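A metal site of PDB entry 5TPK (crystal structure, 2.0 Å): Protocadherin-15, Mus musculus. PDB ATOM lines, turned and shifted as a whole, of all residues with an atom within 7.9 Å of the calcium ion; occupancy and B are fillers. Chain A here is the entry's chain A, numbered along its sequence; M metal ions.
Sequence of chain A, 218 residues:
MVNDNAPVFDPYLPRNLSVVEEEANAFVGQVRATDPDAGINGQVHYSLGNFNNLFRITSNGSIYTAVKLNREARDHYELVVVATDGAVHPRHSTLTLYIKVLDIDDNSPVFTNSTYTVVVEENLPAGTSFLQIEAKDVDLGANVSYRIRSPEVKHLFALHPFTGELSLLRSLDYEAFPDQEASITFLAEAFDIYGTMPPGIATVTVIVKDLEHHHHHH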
ATOM      1  N   ASN A   3      -6.443 -17.962  -6.102  1.00  0.00           N
ATOM      2  CA  ASN A   3      -7.108 -19.229  -5.660  1.00  0.00           C
ATOM      3  C   ASN A   3      -6.343 -20.441  -6.178  1.00  0.00           C
ATOM      4  O   ASN A   3      -6.752 -21.094  -7.143  1.00  0.00           O
ATOM      5  CB  ASN A   3      -8.586 -19.263  -6.094  1.00  0.00           C
ATOM      6  CG  ASN A   3      -9.404 -20.330  -5.364  1.00  0.00           C
ATOM      7  OD1 ASN A   3      -9.238 -20.537  -4.166  1.00  0.00           O
ATOM      8  ND2 ASN A   3     -10.302 -20.997  -6.084  1.00  0.00           N
ATOM      9  N   ASP A   4      -5.211 -20.723  -5.532  1.00  0.00           N
ATOM     10  CA  ASP A   4      -4.315 -21.813  -5.948  1.00  0.00           C
ATOM     11  C   ASP A   4      -4.734 -23.207  -5.451  1.00  0.00           C
ATOM     12  O   ASP A   4      -4.322 -24.212  -6.040  1.00  0.00           O
ATOM     13  CB  ASP A   4      -2.869 -21.524  -5.500  1.00  0.00           C
ATOM     14  CG  ASP A   4      -2.195 -20.448  -6.346  1.00  0.00           C
ATOM     15  OD1 ASP A   4      -2.902 -19.584  -6.910  1.00  0.00           O
ATOM     16  OD2 ASP A   4      -0.949 -20.466  -6.427  1.00  0.00           O
ATOM     17  N   ASN A   5      -5.535 -23.279  -4.386  1.00  0.00           N
ATOM     18  CA  ASN A   5      -5.857 -24.560  -3.760  1.00  0.00           C
ATOM     19  C   ASN A   5      -7.256 -24.631  -3.152  1.00  0.00           C
ATOM     20  O   ASN A   5      -7.898 -23.597  -2.901  1.00  0.00           O
ATOM     21  CB  ASN A   5      -4.800 -24.926  -2.699  1.00  0.00           C
ATOM     22  CG  ASN A   5      -4.389 -23.733  -1.839  1.00  0.00           C
ATOM     23  OD1 ASN A   5      -5.034 -23.424  -0.847  1.00  0.00           O
ATOM     24  ND2 ASN A   5      -3.291 -23.072  -2.231  1.00  0.00           N
ATOM     25  N   ALA A   6      -7.723 -25.858  -2.946  1.00  0.00           N
ATOM     26  CA  ALA A   6      -9.031 -26.141  -2.351  1.00  0.00           C
ATOM     27  C   ALA A   6      -8.909 -26.198  -0.828  1.00  0.00           C
ATOM     28  O   ALA A   6      -7.796 -26.240  -0.296  1.00  0.00           O
ATOM     29  CB  ALA A   6      -9.569 -27.463  -2.861  1.00  0.00           C
ATOM     30  N   PRO A   7     -10.057 -26.189  -0.131  1.00  0.00           N
ATOM     31  CA  PRO A   7     -10.051 -26.543   1.290  1.00  0.00           C
ATOM     32  C   PRO A   7      -9.560 -27.986   1.516  1.00  0.00           C
ATOM     33  O   PRO A   7      -9.932 -28.887   0.756  1.00  0.00           O
ATOM     34  CB  PRO A   7     -11.530 -26.405   1.677  1.00  0.00           C
ATOM     35  CG  PRO A   7     -12.080 -25.411   0.720  1.00  0.00           C
ATOM     36  CD  PRO A   7     -11.374 -25.696  -0.567  1.00  0.00           C
ATOM     37  N   THR A  34      -9.062 -26.185   6.397  1.00  0.00           N
ATOM     38  CA  THR A  34      -8.279 -24.951   6.225  1.00  0.00           C
ATOM     39  C   THR A  34      -8.013 -24.722   4.753  1.00  0.00           C
ATOM     40  O   THR A  34      -7.948 -25.679   3.967  1.00  0.00           O
ATOM     41  CB  THR A  34      -6.927 -25.025   6.946  1.00  0.00           C
ATOM     42  OG1 THR A  34      -6.176 -26.148   6.471  1.00  0.00           O
ATOM     43  CG2 THR A  34      -7.104 -25.148   8.456  1.00  0.00           C
ATOM     44  N   ASP A  35      -7.860 -23.459   4.371  1.00  0.00           N
ATOM     45  CA  ASP A  35      -7.514 -23.079   3.014  1.00  0.00           C
ATOM     46  C   ASP A  35      -6.398 -22.037   3.089  1.00  0.00           C
ATOM     47  O   ASP A  35      -6.686 -20.849   3.263  1.00  0.00           O
ATOM     48  CB  ASP A  35      -8.749 -22.559   2.289  1.00  0.00           C
ATOM     49  CG  ASP A  35      -8.608 -22.561   0.786  1.00  0.00           C
ATOM     50  OD1 ASP A  35      -7.653 -21.955   0.227  1.00  0.00           O
ATOM     51  OD2 ASP A  35      -9.471 -23.166   0.123  1.00  0.00           O
ATOM     52  N   PRO A  36      -5.120 -22.479   3.008  1.00  0.00           N
ATOM     53  CA  PRO A  36      -4.004 -21.532   2.928  1.00  0.00           C
ATOM     54  C   PRO A  36      -4.026 -20.718   1.628  1.00  0.00           C
ATOM     55  O   PRO A  36      -3.343 -21.050   0.666  1.00  0.00           O
ATOM     56  CB  PRO A  36      -2.761 -22.429   3.050  1.00  0.00           C
ATOM     57  CG  PRO A  36      -3.245 -23.655   3.759  1.00  0.00           C
ATOM     58  CD  PRO A  36      -4.643 -23.853   3.255  1.00  0.00           C
ATOM     59  N   ASP A  37      -4.859 -19.688   1.621  1.00  0.00           N
ATOM     60  CA  ASP A  37      -4.920 -18.672   0.561  1.00  0.00           C
ATOM     61  C   ASP A  37      -5.299 -17.373   1.243  1.00  0.00           C
ATOM     62  O   ASP A  37      -5.789 -17.383   2.379  1.00  0.00           O
ATOM     63  CB  ASP A  37      -5.979 -19.025  -0.494  1.00  0.00           C
ATOM     64  CG  ASP A  37      -5.447 -19.929  -1.617  1.00  0.00           C
ATOM     65  OD1 ASP A  37      -4.228 -19.968  -1.875  1.00  0.00           O
ATOM     66  OD2 ASP A  37      -6.279 -20.597  -2.273  1.00  0.00           O
ATOM     67  N   ALA A  38      -5.101 -16.260   0.550  1.00  0.00           N
ATOM     68  CA  ALA A  38      -5.337 -14.924   1.100  1.00  0.00           C
ATOM     69  C   ALA A  38      -6.800 -14.489   0.916  1.00  0.00           C
ATOM     70  O   ALA A  38      -7.383 -14.721  -0.144  1.00  0.00           O
ATOM     71  CB  ALA A  38      -4.400 -13.919   0.465  1.00  0.00           C
ATOM     72  N   ILE A  40     -10.576 -14.045   0.556  1.00  0.00           N
ATOM     73  CA  ILE A  40     -11.818 -14.754   0.217  1.00  0.00           C
ATOM     74  C   ILE A  40     -11.553 -16.121  -0.439  1.00  0.00           C
ATOM     75  O   ILE A  40     -12.414 -17.008  -0.431  1.00  0.00           O
ATOM     76  CB  ILE A  40     -12.756 -13.839  -0.649  1.00  0.00           C
ATOM     77  CG1 ILE A  40     -13.415 -12.752   0.231  1.00  0.00           C
ATOM     78  CG2 ILE A  40     -13.868 -14.622  -1.325  1.00  0.00           C
ATOM     79  CD1 ILE A  40     -12.481 -11.672   0.720  1.00  0.00           C
ATOM     80  N   ASN A  41     -10.353 -16.298  -0.988  1.00  0.00           N
ATOM     81  CA  ASN A  41      -9.915 -17.609  -1.477  1.00  0.00           C
ATOM     82  C   ASN A  41      -9.526 -18.560  -0.333  1.00  0.00           C
ATOM     83  O   ASN A  41      -9.488 -19.777  -0.526  1.00  0.00           O
ATOM     84  CB  ASN A  41      -8.736 -17.458  -2.442  1.00  0.00           C
ATOM     85  CG  ASN A  41      -9.083 -16.606  -3.657  1.00  0.00           C
ATOM     86  OD1 ASN A  41     -10.243 -16.455  -4.027  1.00  0.00           O
ATOM     87  ND2 ASN A  41      -8.049 -16.037  -4.285  1.00  0.00           N
ATOM     88  N   GLY A  42      -9.234 -17.995   0.849  1.00  0.00           N
ATOM     89  CA  GLY A  42      -8.941 -18.765   2.069  1.00  0.00           C
ATOM     90  C   GLY A  42     -10.094 -18.968   3.049  1.00  0.00           C
ATOM     91  O   GLY A  42      -9.901 -19.627   4.077  1.00  0.00           O
ATOM     92  N   GLN A  43     -11.272 -18.409   2.757  1.00  0.00           N
ATOM     93  CA  GLN A  43     -12.436 -18.543   3.645  1.00  0.00           C
ATOM     94  C   GLN A  43     -13.305 -19.773   3.313  1.00  0.00           C
ATOM     95  O   GLN A  43     -13.781 -19.936   2.192  1.00  0.00           O
ATOM     96  CB  GLN A  43     -13.278 -17.257   3.674  1.00  0.00           C
ATOM     97  CG  GLN A  43     -14.081 -16.945   2.420  1.00  0.00           C
ATOM     98  CD  GLN A  43     -15.029 -15.782   2.602  1.00  0.00           C
ATOM     99  OE1 GLN A  43     -16.226 -15.905   2.343  1.00  0.00           O
ATOM    100  NE2 GLN A  43     -14.509 -14.644   3.068  1.00  0.00           N
ATOM    101  N   VAL A  44     -13.518 -20.609   4.318  1.00  0.00           N
ATOM    102  CA  VAL A  44     -14.183 -21.912   4.138  1.00  0.00           C
ATOM    103  C   VAL A  44     -15.642 -21.844   4.567  1.00  0.00           C
ATOM    104  O   VAL A  44     -15.941 -21.370   5.644  1.00  0.00           O
ATOM    105  CB  VAL A  44     -13.433 -22.984   4.957  1.00  0.00           C
ATOM    106  CG1 VAL A  44     -14.118 -24.343   4.818  1.00  0.00           C
ATOM    107  CG2 VAL A  44     -11.967 -23.033   4.527  1.00  0.00           C
ATOM    108  N   THR A  84     -16.377 -25.618   0.928  1.00  0.00           N
ATOM    109  CA  THR A  84     -16.224 -24.791  -0.276  1.00  0.00           C
ATOM    110  C   THR A  84     -15.540 -23.487   0.109  1.00  0.00           C
ATOM    111  O   THR A  84     -15.895 -22.876   1.129  1.00  0.00           O
ATOM    112  CB  THR A  84     -17.618 -24.461  -0.849  1.00  0.00           C
ATOM    113  OG1 THR A  84     -18.324 -25.674  -1.143  1.00  0.00           O
ATOM    114  CG2 THR A  84     -17.510 -23.640  -2.110  1.00  0.00           C
ATOM    115  N   ASP A  85     -14.572 -23.031  -0.690  1.00  0.00           N
ATOM    116  CA  ASP A  85     -13.995 -21.698  -0.462  1.00  0.00           C
ATOM    117  C   ASP A  85     -14.890 -20.599  -1.044  1.00  0.00           C
ATOM    118  O   ASP A  85     -15.826 -20.881  -1.814  1.00  0.00           O
ATOM    119  CB  ASP A  85     -12.535 -21.575  -0.955  1.00  0.00           C
ATOM    120  CG  ASP A  85     -12.380 -21.752  -2.459  1.00  0.00           C
ATOM    121  OD1 ASP A  85     -13.323 -21.449  -3.227  1.00  0.00           O
ATOM    122  OD2 ASP A  85     -11.285 -22.180  -2.883  1.00  0.00           O
ATOM    123  N   GLY A  86     -14.598 -19.349  -0.695  1.00  0.00           N
ATOM    124  CA  GLY A  86     -15.332 -18.191  -1.209  1.00  0.00           C
ATOM    125  C   GLY A  86     -14.900 -17.628  -2.557  1.00  0.00           C
ATOM    126  O   GLY A  86     -15.457 -16.626  -3.004  1.00  0.00           O
ATOM    127  N   ALA A  87     -13.922 -18.257  -3.231  1.00  0.00           N
ATOM    128  CA  ALA A  87     -13.419 -17.762  -4.514  1.00  0.00           C
ATOM    129  C   ALA A  87     -14.497 -17.632  -5.589  1.00  0.00           C
ATOM    130  O   ALA A  87     -15.549 -18.285  -5.514  1.00  0.00           O
ATOM    131  CB  ALA A  87     -12.292 -18.645  -5.030  1.00  0.00           C
ATOM    132  N   HIS A  89     -14.380 -18.573  -8.737  1.00  0.00           N
ATOM    133  CA  HIS A  89     -14.514 -19.940  -9.252  1.00  0.00           C
ATOM    134  C   HIS A  89     -14.320 -20.866  -8.049  1.00  0.00           C
ATOM    135  O   HIS A  89     -13.185 -21.178  -7.693  1.00  0.00           O
ATOM    136  CB  HIS A  89     -13.473 -20.216 -10.342  1.00  0.00           C
ATOM    137  CG  HIS A  89     -13.720 -19.514 -11.640  1.00  0.00           C
ATOM    138  ND1 HIS A  89     -14.408 -20.091 -12.688  1.00  0.00           N
ATOM    139  CD2 HIS A  89     -13.372 -18.276 -12.068  1.00  0.00           C
ATOM    140  CE1 HIS A  89     -14.463 -19.247 -13.698  1.00  0.00           C
ATOM    141  NE2 HIS A  89     -13.853 -18.139 -13.350  1.00  0.00           N
ATOM    142  N   PRO A  90     -15.425 -21.273  -7.372  1.00  0.00           N
ATOM    143  CA  PRO A  90     -15.247 -22.003  -6.105  1.00  0.00           C
ATOM    144  C   PRO A  90     -14.608 -23.387  -6.258  1.00  0.00           C
ATOM    145  O   PRO A  90     -14.826 -24.074  -7.254  1.00  0.00           O
ATOM    146  CB  PRO A  90     -16.687 -22.134  -5.562  1.00  0.00           C
ATOM    147  CG  PRO A  90     -17.504 -21.166  -6.326  1.00  0.00           C
ATOM    148  CD  PRO A  90     -16.854 -21.050  -7.670  1.00  0.00           C
ATOM    149  N   ARG A  91     -13.820 -23.755  -5.245  1.00  0.00           N
ATOM    150  CA  ARG A  91     -13.201 -25.071  -5.137  1.00  0.00           C
ATOM    151  C   ARG A  91     -13.732 -25.799  -3.891  1.00  0.00           C
ATOM    152  O   ARG A  91     -13.772 -25.224  -2.794  1.00  0.00           O
ATOM    153  CB  ARG A  91     -11.682 -24.942  -5.070  1.00  0.00           C
ATOM    154  CG  ARG A  91     -11.070 -24.348  -6.335  1.00  0.00           C
ATOM    155  CD  ARG A  91      -9.581 -24.082  -6.184  1.00  0.00           C
ATOM    156  NE  ARG A  91      -8.798 -25.317  -6.100  1.00  0.00           N
ATOM    157  CZ  ARG A  91      -7.779 -25.684  -6.879  1.00  0.00           C
ATOM    158  NH1 ARG A  91      -7.326 -24.910  -7.886  1.00  0.00           N
ATOM    159  NH2 ARG A  91      -7.183 -26.845  -6.658  1.00  0.00           N
HETATM  160 CA    CA M   1      -8.674 -21.536  -2.098  1.00  0.00          CA
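The backbone carbonyl oxygen (O) of Pro 36 sits close to the side-chain amide oxygen (OD1) of Asn 5, at 3.3 Å.
The backbone carbonyl oxygen of His 89 is in hydrogen-bond range of the side-chain amide nitrogen of Asn 3.
OD2 of Asp 37 sits close to N of Asp 4, at 3.4 Å.
The side-chain carboxylate of Asp 85 lies within hydrogen-bond range of the backbone NH of Arg 91.
OD1 of Asp 85 sits at hydrogen-bond distance from N of Ala 87 (3.2 Å).
Six residues have an atom within 4 Å of the calcium ion: Asn 3, Asn 5, Asp 35, Asp 37, Asn 41 and Asp 85.
The nearest printed residue that does not touch the calcium ion is Ala 6 (4.5 Å).
The calcium ion is bound by the backbone carbonyl oxygen (O) of Asn 5 (2.3 Å), the side-chain amide oxygen (OD1) of Asn 3 (2.4 Å), the backbone carbonyl oxygen (O) of Asn 41 (2.5 Å), the side-chain carboxylate (OD1) of Asp 35 (2.6 Å), the side-chain carboxylate (OD2) of Asp 37 (2.6 Å), the side-chain carboxylate (OD2) of Asp 85 (2.8 Å) and the side-chain carboxylate (OD2) of Asp 35 (2.9 Å).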
